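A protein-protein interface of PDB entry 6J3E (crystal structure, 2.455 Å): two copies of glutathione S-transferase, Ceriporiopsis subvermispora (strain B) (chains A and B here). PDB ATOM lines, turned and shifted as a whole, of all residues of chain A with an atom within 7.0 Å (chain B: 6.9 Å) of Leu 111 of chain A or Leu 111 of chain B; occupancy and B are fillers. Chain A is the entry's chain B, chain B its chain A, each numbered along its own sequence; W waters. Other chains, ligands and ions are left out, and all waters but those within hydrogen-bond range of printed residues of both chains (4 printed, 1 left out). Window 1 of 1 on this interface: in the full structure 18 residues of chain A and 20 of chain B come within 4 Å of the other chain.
A ring nitrogen (ND1) of His 112 of chain B is in hydrogen-bond range of the backbone carbonyl oxygen of Thr 108 of chain B (3.1 Å).
Among the printed residues, merely in contact across the chains: Leu 200 of chain A with Glu 107 of chain B (3.0 Å), Ala 110 of chain A with Trp 188 of chain B (3.2 Å), Trp 188 of chain A with Ala 110 of chain B (3.3 Å), Glu 107 of chain A with Leu 200 of chain B (3.3 Å), Phe 199 of chain A with Ala 110 of chain B (3.4 Å), Phe 117 of chain A with Trp 188 of chain B (3.5 Å), Trp 188 of chain A with Ala 114 of chain B (3.5 Å), Ala 110 of chain A with Phe 199 of chain B (3.5 Å), Ala 113 of chain A with Trp 188 of chain B (3.6 Å), Glu 107 of chain A with Phe 199 of chain B (3.6 Å), Trp 188 of chain A with Ala 113 of chain B (3.7 Å), Ala 114 of chain A with Trp 188 of chain B (3.7 Å), Phe 199 of chain A with Leu 111 of chain B (3.7 Å), Phe 199 of chain A with Glu 107 of chain B (3.7 Å), Ala 114 of chain A with Phe 115 of chain B (3.8 Å), Leu 111 of chain A with Phe 115 of chain B (3.8 Å), Phe 115 of chain A with Leu 111 of chain B (3.8 Å), Leu 111 of chain A with Phe 199 of chain B (3.8 Å), Leu 111 of chain A with Leu 111 of chain B (3.9 Å), Leu 111 of chain A with Thr 108 of chain B (3.9 Å) and Ala 110 of chain A with Leu 189 of chain B (3.97 Å).
Of the printed residues of chain B, Glu 107 of chain A touches Phe 199 and Leu 200. Of chain B, only Thr 108 (3.9 Å), Leu 111 (3.9 Å), Phe 115 (3.8 Å) and Phe 199 (3.8 Å) come within 4 Å of Leu 111 of chain A. Of the printed residues of chain A, Glu 107 of chain B touches Phe 199 and Leu 200. Printed residues of chain A within 4 Å of Ala 110 of chain B: Trp 188 (3.3 Å) and Phe 199 (3.4 Å). Printed residues of chain A within 4 Å of Phe 115 of chain B: Leu 111 (3.8 Å) and Ala 114 (3.8 Å). Printed residues of chain A within 4 Å of Leu 200 of chain B: Glu 107. The nearest residue of chain B that does not touch Leu 111 of chain A is His 112 of chain B (4.1 Å). The nearest printed residue of chain A that does not touch Leu 111 of chain B is Leu 200 of chain A (4.01 Å).
Hydrophobic or aromatic side chains of chain B that line the printed part of chain A: Ala 110, Leu 111, Ala 113, Ala 114, Phe 115, Trp 188, Leu 189, Phe 199 and Leu 200. Hydrophobic or aromatic side chains of chain A that line the printed part of chain B: Ala 110, Leu 111, Ala 113, Ala 114, Phe 115, Phe 117, Trp 188, Phe 199 and Leu 200. Among the printed residues, 21 pairs touch across the chains. Among the printed residues, no Asp or Glu carboxylate lies within 4 Å of a Lys or Arg side-chain nitrogen of the other chain.
Leu 111 of chain B touches its own counterpart, Leu 111 of chain A. Leu 111 of chain A touches Phe 115 of chain B, and with the chains exchanged Phe 115 of chain A touches Leu 111 of chain B. Leu 111 of chain A touches Phe 199 of chain B, and with the chains exchanged Phe 199 of chain A touches Leu 111 of chain B. Ala 114 of chain A touches Phe 115 of chain B, but with the chains exchanged Phe 115 of chain A does not touch Ala 114 of chain B (4.03 Å). 17 positions are printed for both chains. Of the 21 pairs that touch across the chains among the printed residues, 17 have their exchanged pair printed and touching as well.
Water W1 lies within hydrogen-bond range of OD1 of Asp 109 of chain B (2.5 Å), O of Trp 188 of chain A (2.8 Å) and N of Ala 110 of chain B (3.5 Å). Water W2 lies within hydrogen-bond range of the backbone carbonyl oxygen (O) of Phe 199 of chain A (2.5 Å), the backbone carbonyl oxygen (O) of Glu 107 of chain B (2.5 Å) and the backbone NH (N) of Leu 111 of chain B (3.2 Å). Water W3 lies within hydrogen-bond range of the backbone NH (N) of Ala 110 of chain A (2.7 Å), the backbone carbonyl oxygen (O) of Phe 199 of chain B (2.8 Å), the backbone carbonyl oxygen (O) of Pro 106 of chain A (3.0 Å) and the backbone NH (N) of Asp 109 of chain A (3.1 Å).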
ATOM      1  N   PRO A 106     -24.909 -11.619 -33.022  1.00  0.00           N
ATOM      2  CA  PRO A 106     -23.525 -11.329 -33.437  1.00  0.00           C
ATOM      3  C   PRO A 106     -22.996  -9.990 -32.959  1.00  0.00           C
ATOM      4  O   PRO A 106     -21.856  -9.917 -32.487  1.00  0.00           O
ATOM      5  CB  PRO A 106     -23.617 -11.374 -34.966  1.00  0.00           C
ATOM      6  CG  PRO A 106     -24.719 -12.342 -35.231  1.00  0.00           C
ATOM      7  CD  PRO A 106     -25.716 -12.185 -34.117  1.00  0.00           C
ATOM      8  N   GLU A 107     -23.791  -8.924 -33.088  1.00  0.00           N
ATOM      9  CA  GLU A 107     -23.349  -7.606 -32.653  1.00  0.00           C
ATOM     10  C   GLU A 107     -23.004  -7.586 -31.162  1.00  0.00           C
ATOM     11  O   GLU A 107     -22.254  -6.705 -30.726  1.00  0.00           O
ATOM     12  CB  GLU A 107     -24.427  -6.562 -32.989  1.00  0.00           C
ATOM     13  CG  GLU A 107     -25.579  -6.483 -31.989  1.00  0.00           C
ATOM     14  CD  GLU A 107     -26.823  -7.274 -32.427  1.00  0.00           C
ATOM     15  OE1 GLU A 107     -27.949  -6.921 -31.993  1.00  0.00           O
ATOM     16  OE2 GLU A 107     -26.670  -8.247 -33.209  1.00  0.00           O
ATOM     17  N   THR A 108     -23.511  -8.548 -30.382  1.00  0.00           N
ATOM     18  CA  THR A 108     -23.256  -8.637 -28.949  1.00  0.00           C
ATOM     19  C   THR A 108     -22.288  -9.748 -28.591  1.00  0.00           C
ATOM     20  O   THR A 108     -22.151 -10.056 -27.400  1.00  0.00           O
ATOM     21  CB  THR A 108     -24.554  -8.871 -28.158  1.00  0.00           C
ATOM     22  OG1 THR A 108     -24.943 -10.252 -28.258  1.00  0.00           O
ATOM     23  CG2 THR A 108     -25.673  -7.997 -28.659  1.00  0.00           C
ATOM     24  N   ASP A 109     -21.628 -10.366 -29.580  1.00  0.00           N
ATOM     25  CA  ASP A 109     -20.801 -11.537 -29.287  1.00  0.00           C
ATOM     26  C   ASP A 109     -19.625 -11.179 -28.379  1.00  0.00           C
ATOM     27  O   ASP A 109     -19.382 -11.851 -27.370  1.00  0.00           O
ATOM     28  CB  ASP A 109     -20.293 -12.189 -30.573  1.00  0.00           C
ATOM     29  CG  ASP A 109     -19.571 -13.500 -30.299  1.00  0.00           C
ATOM     30  OD1 ASP A 109     -18.359 -13.480 -30.020  1.00  0.00           O
ATOM     31  OD2 ASP A 109     -20.227 -14.561 -30.306  1.00  0.00           O
ATOM     32  N   ALA A 110     -18.882 -10.121 -28.722  1.00  0.00           N
ATOM     33  CA  ALA A 110     -17.712  -9.747 -27.939  1.00  0.00           C
ATOM     34  C   ALA A 110     -18.092  -9.184 -26.568  1.00  0.00           C
ATOM     35  O   ALA A 110     -17.355  -9.391 -25.596  1.00  0.00           O
ATOM     36  CB  ALA A 110     -16.867  -8.743 -28.720  1.00  0.00           C
ATOM     37  N   LEU A 111     -19.223  -8.472 -26.455  1.00  0.00           N
ATOM     38  CA  LEU A 111     -19.666  -8.048 -25.127  1.00  0.00           C
ATOM     39  C   LEU A 111     -20.050  -9.248 -24.262  1.00  0.00           C
ATOM     40  O   LEU A 111     -19.830  -9.233 -23.049  1.00  0.00           O
ATOM     41  CB  LEU A 111     -20.832  -7.061 -25.240  1.00  0.00           C
ATOM     42  CG  LEU A 111     -20.487  -5.637 -25.699  1.00  0.00           C
ATOM     43  CD1 LEU A 111     -21.724  -4.807 -26.038  1.00  0.00           C
ATOM     44  CD2 LEU A 111     -19.727  -4.955 -24.615  1.00  0.00           C
ATOM     45  N   HIS A 112     -20.618 -10.296 -24.862  1.00  0.00           N
ATOM     46  CA  HIS A 112     -20.857 -11.538 -24.128  1.00  0.00           C
ATOM     47  C   HIS A 112     -19.541 -12.146 -23.627  1.00  0.00           C
ATOM     48  O   HIS A 112     -19.469 -12.669 -22.501  1.00  0.00           O
ATOM     49  CB  HIS A 112     -21.626 -12.534 -25.014  1.00  0.00           C
ATOM     50  CG  HIS A 112     -23.110 -12.511 -24.817  1.00  0.00           C
ATOM     51  ND1 HIS A 112     -23.953 -11.730 -25.581  1.00  0.00           N
ATOM     52  CD2 HIS A 112     -23.905 -13.170 -23.937  1.00  0.00           C
ATOM     53  CE1 HIS A 112     -25.200 -11.901 -25.176  1.00  0.00           C
ATOM     54  NE2 HIS A 112     -25.199 -12.772 -24.181  1.00  0.00           N
ATOM     55  N   ALA A 113     -18.478 -12.071 -24.431  1.00  0.00           N
ATOM     56  CA  ALA A 113     -17.190 -12.567 -23.953  1.00  0.00           C
ATOM     57  C   ALA A 113     -16.675 -11.731 -22.781  1.00  0.00           C
ATOM     58  O   ALA A 113     -16.123 -12.276 -21.818  1.00  0.00           O
ATOM     59  CB  ALA A 113     -16.173 -12.585 -25.092  1.00  0.00           C
ATOM     60  N   ALA A 114     -16.854 -10.407 -22.844  1.00  0.00           N
ATOM     61  CA  ALA A 114     -16.482  -9.541 -21.726  1.00  0.00           C
ATOM     62  C   ALA A 114     -17.353  -9.819 -20.516  1.00  0.00           C
ATOM     63  O   ALA A 114     -16.867  -9.805 -19.376  1.00  0.00           O
ATOM     64  CB  ALA A 114     -16.601  -8.065 -22.119  1.00  0.00           C
ATOM     65  N   PHE A 115     -18.645 -10.075 -20.748  1.00  0.00           N
ATOM     66  CA  PHE A 115     -19.546 -10.362 -19.642  1.00  0.00           C
ATOM     67  C   PHE A 115     -19.114 -11.630 -18.922  1.00  0.00           C
ATOM     68  O   PHE A 115     -19.087 -11.672 -17.687  1.00  0.00           O
ATOM     69  CB  PHE A 115     -20.992 -10.471 -20.145  1.00  0.00           C
ATOM     70  CG  PHE A 115     -21.909 -11.200 -19.195  1.00  0.00           C
ATOM     71  CD1 PHE A 115     -22.585 -10.519 -18.192  1.00  0.00           C
ATOM     72  CD2 PHE A 115     -22.075 -12.566 -19.290  1.00  0.00           C
ATOM     73  CE1 PHE A 115     -23.412 -11.195 -17.300  1.00  0.00           C
ATOM     74  CE2 PHE A 115     -22.877 -13.247 -18.400  1.00  0.00           C
ATOM     75  CZ  PHE A 115     -23.548 -12.564 -17.407  1.00  0.00           C
ATOM     76  N   ASN A 116     -18.753 -12.672 -19.677  1.00  0.00           N
ATOM     77  CA  ASN A 116     -18.317 -13.909 -19.040  1.00  0.00           C
ATOM     78  C   ASN A 116     -17.139 -13.673 -18.094  1.00  0.00           C
ATOM     79  O   ASN A 116     -17.126 -14.197 -16.972  1.00  0.00           O
ATOM     80  CB  ASN A 116     -17.964 -14.971 -20.079  1.00  0.00           C
ATOM     81  CG  ASN A 116     -17.622 -16.285 -19.420  1.00  0.00           C
ATOM     82  OD1 ASN A 116     -18.483 -16.956 -18.852  1.00  0.00           O
ATOM     83  ND2 ASN A 116     -16.350 -16.622 -19.421  1.00  0.00           N
ATOM     84  N   PHE A 117     -16.158 -12.858 -18.503  1.00  0.00           N
ATOM     85  CA  PHE A 117     -15.069 -12.534 -17.582  1.00  0.00           C
ATOM     86  C   PHE A 117     -15.583 -11.737 -16.388  1.00  0.00           C
ATOM     87  O   PHE A 117     -15.256 -12.050 -15.238  1.00  0.00           O
ATOM     88  CB  PHE A 117     -13.950 -11.768 -18.290  1.00  0.00           C
ATOM     89  CG  PHE A 117     -12.852 -11.323 -17.363  1.00  0.00           C
ATOM     90  CD1 PHE A 117     -12.096 -12.255 -16.664  1.00  0.00           C
ATOM     91  CD2 PHE A 117     -12.586  -9.973 -17.168  1.00  0.00           C
ATOM     92  CE1 PHE A 117     -11.091 -11.842 -15.781  1.00  0.00           C
ATOM     93  CE2 PHE A 117     -11.585  -9.557 -16.295  1.00  0.00           C
ATOM     94  CZ  PHE A 117     -10.841 -10.489 -15.599  1.00  0.00           C
ATOM     95  N   TRP A 188     -25.602  -3.340 -13.216  1.00  0.00           N
ATOM     96  CA  TRP A 188     -25.493  -3.457 -14.671  1.00  0.00           C
ATOM     97  C   TRP A 188     -26.862  -3.519 -15.331  1.00  0.00           C
ATOM     98  O   TRP A 188     -27.076  -2.912 -16.385  1.00  0.00           O
ATOM     99  CB  TRP A 188     -24.700  -4.701 -15.076  1.00  0.00           C
ATOM    100  CG  TRP A 188     -23.379  -4.851 -14.430  1.00  0.00           C
ATOM    101  CD1 TRP A 188     -22.660  -3.889 -13.816  1.00  0.00           C
ATOM    102  CD2 TRP A 188     -22.613  -6.059 -14.335  1.00  0.00           C
ATOM    103  NE1 TRP A 188     -21.492  -4.413 -13.330  1.00  0.00           N
ATOM    104  CE2 TRP A 188     -21.438  -5.747 -13.632  1.00  0.00           C
ATOM    105  CE3 TRP A 188     -22.811  -7.374 -14.777  1.00  0.00           C
ATOM    106  CZ2 TRP A 188     -20.449  -6.701 -13.355  1.00  0.00           C
ATOM    107  CZ3 TRP A 188     -21.840  -8.323 -14.501  1.00  0.00           C
ATOM    108  CH2 TRP A 188     -20.673  -7.981 -13.789  1.00  0.00           C
ATOM    109  N   LEU A 189     -27.789  -4.276 -14.745  1.00  0.00           N
ATOM    110  CA  LEU A 189     -29.099  -4.478 -15.358  1.00  0.00           C
ATOM    111  C   LEU A 189     -29.995  -3.261 -15.236  1.00  0.00           C
ATOM    112  O   LEU A 189     -31.102  -3.267 -15.786  1.00  0.00           O
ATOM    113  CB  LEU A 189     -29.803  -5.685 -14.732  1.00  0.00           C
ATOM    114  CG  LEU A 189     -29.285  -7.022 -15.243  1.00  0.00           C
ATOM    115  CD1 LEU A 189     -29.802  -8.186 -14.403  1.00  0.00           C
ATOM    116  CD2 LEU A 189     -29.669  -7.167 -16.699  1.00  0.00           C
ATOM    117  N   PHE A 199     -30.599  -8.985 -20.079  1.00  0.00           N
ATOM    118  CA  PHE A 199     -29.540  -8.057 -20.452  1.00  0.00           C
ATOM    119  C   PHE A 199     -29.891  -7.253 -21.697  1.00  0.00           C
ATOM    120  O   PHE A 199     -29.622  -6.049 -21.749  1.00  0.00           O
ATOM    121  CB  PHE A 199     -28.238  -8.824 -20.637  1.00  0.00           C
ATOM    122  CG  PHE A 199     -27.373  -8.791 -19.421  1.00  0.00           C
ATOM    123  CD1 PHE A 199     -27.647  -9.621 -18.345  1.00  0.00           C
ATOM    124  CD2 PHE A 199     -26.330  -7.906 -19.330  1.00  0.00           C
ATOM    125  CE1 PHE A 199     -26.903  -9.581 -17.218  1.00  0.00           C
ATOM    126  CE2 PHE A 199     -25.588  -7.868 -18.204  1.00  0.00           C
ATOM    127  CZ  PHE A 199     -25.877  -8.713 -17.139  1.00  0.00           C
ATOM    128  N   LEU A 200     -30.500  -7.892 -22.702  1.00  0.00           N
ATOM    129  CA  LEU A 200     -30.902  -7.231 -23.947  1.00  0.00           C
ATOM    130  C   LEU A 200     -32.230  -6.479 -23.829  1.00  0.00           C
ATOM    131  O   LEU A 200     -32.740  -5.978 -24.837  1.00  0.00           O
ATOM    132  CB  LEU A 200     -30.991  -8.250 -25.096  1.00  0.00           C
ATOM    133  CG  LEU A 200     -29.701  -9.001 -25.482  1.00  0.00           C
ATOM    134  CD1 LEU A 200     -29.809  -9.845 -26.751  1.00  0.00           C
ATOM    135  CD2 LEU A 200     -28.568  -8.030 -25.625  1.00  0.00           C
ATOM    136  N   SER A 205     -30.888 -13.716 -23.699  1.00  0.00           N
ATOM    137  CA  SER A 205     -29.533 -13.820 -24.216  1.00  0.00           C
ATOM    138  C   SER A 205     -28.778 -14.856 -23.403  1.00  0.00           C
ATOM    139  O   SER A 205     -29.232 -15.293 -22.342  1.00  0.00           O
ATOM    140  CB  SER A 205     -28.803 -12.484 -24.146  1.00  0.00           C
ATOM    141  OG  SER A 205     -28.739 -12.083 -22.794  1.00  0.00           O
ATOM    142  N   ALA A 207     -26.181 -14.295 -21.718  1.00  0.00           N
ATOM    143  CA  ALA A 207     -25.822 -13.718 -20.427  1.00  0.00           C
ATOM    144  C   ALA A 207     -26.869 -14.050 -19.359  1.00  0.00           C
ATOM    145  O   ALA A 207     -26.512 -14.457 -18.246  1.00  0.00           O
ATOM    146  CB  ALA A 207     -25.614 -12.210 -20.558  1.00  0.00           C
ATOM    147  N   ARG B  91     -24.164   8.031 -21.770  1.00  0.00           N
ATOM    148  CA  ARG B  91     -25.595   7.750 -21.847  1.00  0.00           C
ATOM    149  C   ARG B  91     -26.388   9.033 -21.948  1.00  0.00           C
ATOM    150  O   ARG B  91     -27.358   9.108 -22.711  1.00  0.00           O
ATOM    151  CB  ARG B  91     -26.065   6.940 -20.641  1.00  0.00           C
ATOM    152  CG  ARG B  91     -25.422   5.562 -20.571  1.00  0.00           C
ATOM    153  CD  ARG B  91     -25.900   4.767 -19.374  1.00  0.00           C
ATOM    154  NE  ARG B  91     -25.567   3.362 -19.499  1.00  0.00           N
ATOM    155  CZ  ARG B  91     -24.376   2.868 -19.232  1.00  0.00           C
ATOM    156  NH1 ARG B  91     -24.172   1.558 -19.368  1.00  0.00           N
ATOM    157  NH2 ARG B  91     -23.363   3.665 -18.827  1.00  0.00           N
ATOM    158  N   PRO B 106     -29.392   0.599 -26.998  1.00  0.00           N
ATOM    159  CA  PRO B 106     -30.090   0.176 -25.768  1.00  0.00           C
ATOM    160  C   PRO B 106     -29.995  -1.309 -25.459  1.00  0.00           C
ATOM    161  O   PRO B 106     -29.924  -1.673 -24.280  1.00  0.00           O
ATOM    162  CB  PRO B 106     -31.543   0.602 -26.035  1.00  0.00           C
ATOM    163  CG  PRO B 106     -31.416   1.747 -26.945  1.00  0.00           C
ATOM    164  CD  PRO B 106     -30.227   1.474 -27.832  1.00  0.00           C
ATOM    165  N   GLU B 107     -30.022  -2.178 -26.476  1.00  0.00           N
ATOM    166  CA  GLU B 107     -29.915  -3.606 -26.215  1.00  0.00           C
ATOM    167  C   GLU B 107     -28.558  -3.986 -25.639  1.00  0.00           C
ATOM    168  O   GLU B 107     -28.419  -5.090 -25.103  1.00  0.00           O
ATOM    169  CB  GLU B 107     -30.160  -4.404 -27.493  1.00  0.00           C
ATOM    170  CG  GLU B 107     -31.609  -4.533 -27.885  1.00  0.00           C
ATOM    171  CD  GLU B 107     -31.839  -5.547 -29.007  1.00  0.00           C
ATOM    172  OE1 GLU B 107     -30.912  -6.329 -29.323  1.00  0.00           O
ATOM    173  OE2 GLU B 107     -32.959  -5.559 -29.565  1.00  0.00           O
ATOM    174  N   THR B 108     -27.563  -3.096 -25.725  1.00  0.00           N
ATOM    175  CA  THR B 108     -26.208  -3.347 -25.239  1.00  0.00           C
ATOM    176  C   THR B 108     -25.900  -2.652 -23.923  1.00  0.00           C
ATOM    177  O   THR B 108     -24.750  -2.692 -23.473  1.00  0.00           O
ATOM    178  CB  THR B 108     -25.173  -2.900 -26.273  1.00  0.00           C
ATOM    179  OG1 THR B 108     -25.201  -1.468 -26.392  1.00  0.00           O
ATOM    180  CG2 THR B 108     -25.458  -3.543 -27.631  1.00  0.00           C
ATOM    181  N   ASP B 109     -26.891  -2.024 -23.290  1.00  0.00           N
ATOM    182  CA  ASP B 109     -26.588  -1.121 -22.185  1.00  0.00           C
ATOM    183  C   ASP B 109     -26.119  -1.883 -20.955  1.00  0.00           C
ATOM    184  O   ASP B 109     -25.121  -1.509 -20.322  1.00  0.00           O
ATOM    185  CB  ASP B 109     -27.804  -0.275 -21.850  1.00  0.00           C
ATOM    186  CG  ASP B 109     -27.540   0.669 -20.715  1.00  0.00           C
ATOM    187  OD1 ASP B 109     -27.587   0.233 -19.546  1.00  0.00           O
ATOM    188  OD2 ASP B 109     -27.274   1.849 -20.996  1.00  0.00           O
ATOM    189  N   ALA B 110     -26.841  -2.947 -20.584  1.00  0.00           N
ATOM    190  CA  ALA B 110     -26.403  -3.764 -19.459  1.00  0.00           C
ATOM    191  C   ALA B 110     -25.087  -4.478 -19.774  1.00  0.00           C
ATOM    192  O   ALA B 110     -24.206  -4.567 -18.915  1.00  0.00           O
ATOM    193  CB  ALA B 110     -27.503  -4.744 -19.069  1.00  0.00           C
ATOM    194  N   LEU B 111     -24.916  -4.949 -21.007  1.00  0.00           N
ATOM    195  CA  LEU B 111     -23.659  -5.578 -21.392  1.00  0.00           C
ATOM    196  C   LEU B 111     -22.500  -4.595 -21.340  1.00  0.00           C
ATOM    197  O   LEU B 111     -21.379  -4.974 -20.964  1.00  0.00           O
ATOM    198  CB  LEU B 111     -23.778  -6.177 -22.787  1.00  0.00           C
ATOM    199  CG  LEU B 111     -24.477  -7.526 -22.778  1.00  0.00           C
ATOM    200  CD1 LEU B 111     -24.819  -7.969 -24.202  1.00  0.00           C
ATOM    201  CD2 LEU B 111     -23.577  -8.536 -22.116  1.00  0.00           C
ATOM    202  N   HIS B 112     -22.745  -3.331 -21.714  1.00  0.00           N
ATOM    203  CA  HIS B 112     -21.715  -2.300 -21.573  1.00  0.00           C
ATOM    204  C   HIS B 112     -21.322  -2.122 -20.116  1.00  0.00           C
ATOM    205  O   HIS B 112     -20.131  -2.059 -19.782  1.00  0.00           O
ATOM    206  CB  HIS B 112     -22.195  -0.969 -22.146  1.00  0.00           C
ATOM    207  CG  HIS B 112     -21.725  -0.702 -23.545  1.00  0.00           C
ATOM    208  ND1 HIS B 112     -22.454  -1.065 -24.660  1.00  0.00           N
ATOM    209  CD2 HIS B 112     -20.602  -0.101 -24.009  1.00  0.00           C
ATOM    210  CE1 HIS B 112     -21.796  -0.701 -25.748  1.00  0.00           C
ATOM    211  NE2 HIS B 112     -20.672  -0.109 -25.382  1.00  0.00           N
ATOM    212  N   ALA B 113     -22.314  -2.026 -19.233  1.00  0.00           N
ATOM    213  CA  ALA B 113     -22.003  -1.858 -17.818  1.00  0.00           C
ATOM    214  C   ALA B 113     -21.194  -3.033 -17.305  1.00  0.00           C
ATOM    215  O   ALA B 113     -20.289  -2.859 -16.478  1.00  0.00           O
ATOM    216  CB  ALA B 113     -23.282  -1.705 -17.002  1.00  0.00           C
ATOM    217  N   ALA B 114     -21.505  -4.241 -17.791  1.00  0.00           N
ATOM    218  CA  ALA B 114     -20.698  -5.396 -17.432  1.00  0.00           C
ATOM    219  C   ALA B 114     -19.310  -5.291 -18.049  1.00  0.00           C
ATOM    220  O   ALA B 114     -18.309  -5.638 -17.414  1.00  0.00           O
ATOM    221  CB  ALA B 114     -21.392  -6.680 -17.871  1.00  0.00           C
ATOM    222  N   PHE B 115     -19.220  -4.798 -19.284  1.00  0.00           N
ATOM    223  CA  PHE B 115     -17.908  -4.646 -19.888  1.00  0.00           C
ATOM    224  C   PHE B 115     -17.050  -3.700 -19.065  1.00  0.00           C
ATOM    225  O   PHE B 115     -15.863  -3.963 -18.839  1.00  0.00           O
ATOM    226  CB  PHE B 115     -18.043  -4.150 -21.328  1.00  0.00           C
ATOM    227  CG  PHE B 115     -16.773  -3.572 -21.888  1.00  0.00           C
ATOM    228  CD1 PHE B 115     -15.823  -4.391 -22.487  1.00  0.00           C
ATOM    229  CD2 PHE B 115     -16.512  -2.200 -21.808  1.00  0.00           C
ATOM    230  CE1 PHE B 115     -14.647  -3.857 -23.006  1.00  0.00           C
ATOM    231  CE2 PHE B 115     -15.329  -1.663 -22.332  1.00  0.00           C
ATOM    232  CZ  PHE B 115     -14.399  -2.495 -22.921  1.00  0.00           C
ATOM    233  N   ASN B 116     -17.638  -2.603 -18.586  1.00  0.00           N
ATOM    234  CA  ASN B 116     -16.870  -1.640 -17.803  1.00  0.00           C
ATOM    235  C   ASN B 116     -16.180  -2.326 -16.627  1.00  0.00           C
ATOM    236  O   ASN B 116     -14.972  -2.163 -16.415  1.00  0.00           O
ATOM    237  CB  ASN B 116     -17.774  -0.506 -17.307  1.00  0.00           C
ATOM    238  CG  ASN B 116     -16.986   0.561 -16.565  1.00  0.00           C
ATOM    239  OD1 ASN B 116     -16.224   1.301 -17.180  1.00  0.00           O
ATOM    240  ND2 ASN B 116     -17.137   0.618 -15.237  1.00  0.00           N
ATOM    241  N   TRP B 188     -11.707 -11.594 -26.340  1.00  0.00           N
ATOM    242  CA  TRP B 188     -13.116 -11.195 -26.394  1.00  0.00           C
ATOM    243  C   TRP B 188     -13.520 -10.743 -27.793  1.00  0.00           C
ATOM    244  O   TRP B 188     -14.631 -11.037 -28.247  1.00  0.00           O
ATOM    245  CB  TRP B 188     -13.407 -10.068 -25.414  1.00  0.00           C
ATOM    246  CG  TRP B 188     -13.073 -10.378 -24.028  1.00  0.00           C
ATOM    247  CD1 TRP B 188     -12.836 -11.604 -23.490  1.00  0.00           C
ATOM    248  CD2 TRP B 188     -12.910  -9.432 -22.970  1.00  0.00           C
ATOM    249  NE1 TRP B 188     -12.539 -11.480 -22.155  1.00  0.00           N
ATOM    250  CE2 TRP B 188     -12.576 -10.154 -21.813  1.00  0.00           C
ATOM    251  CE3 TRP B 188     -13.015  -8.041 -22.892  1.00  0.00           C
ATOM    252  CZ2 TRP B 188     -12.350  -9.535 -20.590  1.00  0.00           C
ATOM    253  CZ3 TRP B 188     -12.783  -7.429 -21.678  1.00  0.00           C
ATOM    254  CH2 TRP B 188     -12.456  -8.177 -20.545  1.00  0.00           C
ATOM    255  N   LEU B 189     -12.638 -10.001 -28.473  1.00  0.00           N
ATOM    256  CA  LEU B 189     -12.937  -9.395 -29.762  1.00  0.00           C
ATOM    257  C   LEU B 189     -12.886 -10.383 -30.912  1.00  0.00           C
ATOM    258  O   LEU B 189     -13.292 -10.014 -32.020  1.00  0.00           O
ATOM    259  CB  LEU B 189     -11.972  -8.246 -30.054  1.00  0.00           C
ATOM    260  CG  LEU B 189     -12.352  -7.037 -29.234  1.00  0.00           C
ATOM    261  CD1 LEU B 189     -11.271  -5.945 -29.319  1.00  0.00           C
ATOM    262  CD2 LEU B 189     -13.726  -6.535 -29.719  1.00  0.00           C
ATOM    263  N   PHE B 199     -16.297  -3.689 -30.874  1.00  0.00           N
ATOM    264  CA  PHE B 199     -17.074  -4.705 -30.166  1.00  0.00           C
ATOM    265  C   PHE B 199     -18.337  -5.115 -30.922  1.00  0.00           C
ATOM    266  O   PHE B 199     -18.663  -6.308 -30.975  1.00  0.00           O
ATOM    267  CB  PHE B 199     -17.412  -4.214 -28.762  1.00  0.00           C
ATOM    268  CG  PHE B 199     -16.412  -4.643 -27.762  1.00  0.00           C
ATOM    269  CD1 PHE B 199     -15.176  -4.004 -27.690  1.00  0.00           C
ATOM    270  CD2 PHE B 199     -16.666  -5.726 -26.941  1.00  0.00           C
ATOM    271  CE1 PHE B 199     -14.219  -4.420 -26.792  1.00  0.00           C
ATOM    272  CE2 PHE B 199     -15.713  -6.147 -26.027  1.00  0.00           C
ATOM    273  CZ  PHE B 199     -14.481  -5.496 -25.957  1.00  0.00           C
ATOM    274  N   LEU B 200     -19.080  -4.145 -31.487  1.00  0.00           N
ATOM    275  CA  LEU B 200     -20.297  -4.450 -32.239  1.00  0.00           C
ATOM    276  C   LEU B 200     -20.025  -4.850 -33.680  1.00  0.00           C
ATOM    277  O   LEU B 200     -20.986  -5.031 -34.435  1.00  0.00           O
ATOM    278  CB  LEU B 200     -21.272  -3.267 -32.253  1.00  0.00           C
ATOM    279  CG  LEU B 200     -21.556  -2.452 -31.000  1.00  0.00           C
ATOM    280  CD1 LEU B 200     -22.429  -1.252 -31.368  1.00  0.00           C
ATOM    281  CD2 LEU B 200     -22.219  -3.297 -29.918  1.00  0.00           C
ATOM    282  N   SER B 205     -18.900   1.837 -30.612  1.00  0.00           N
ATOM    283  CA  SER B 205     -19.685   1.811 -29.390  1.00  0.00           C
ATOM    284  C   SER B 205     -18.860   2.438 -28.279  1.00  0.00           C
ATOM    285  O   SER B 205     -17.656   2.670 -28.432  1.00  0.00           O
ATOM    286  CB  SER B 205     -20.073   0.378 -29.028  1.00  0.00           C
ATOM    287  OG  SER B 205     -18.902  -0.414 -28.975  1.00  0.00           O
ATOM    288  N   ALA B 207     -17.822   0.989 -25.807  1.00  0.00           N
ATOM    289  CA  ALA B 207     -16.814   0.033 -25.347  1.00  0.00           C
ATOM    290  C   ALA B 207     -15.495   0.234 -26.083  1.00  0.00           C
ATOM    291  O   ALA B 207     -14.419   0.105 -25.489  1.00  0.00           O
ATOM    292  CB  ALA B 207     -17.319  -1.403 -25.508  1.00  0.00           C
HETATM  293  O   HOH W   1     -28.696  -1.437 -18.059  1.00  0.00           O
HETATM  294  O   HOH W   2     -27.399  -5.704 -22.856  1.00  0.00           O
HETATM  295  O   HOH W   3     -19.261  -9.082 -31.152  1.00  0.00           O
HETATM  296  O   HOH W   4     -20.309  -6.830 -28.815  1.00  0.00           O
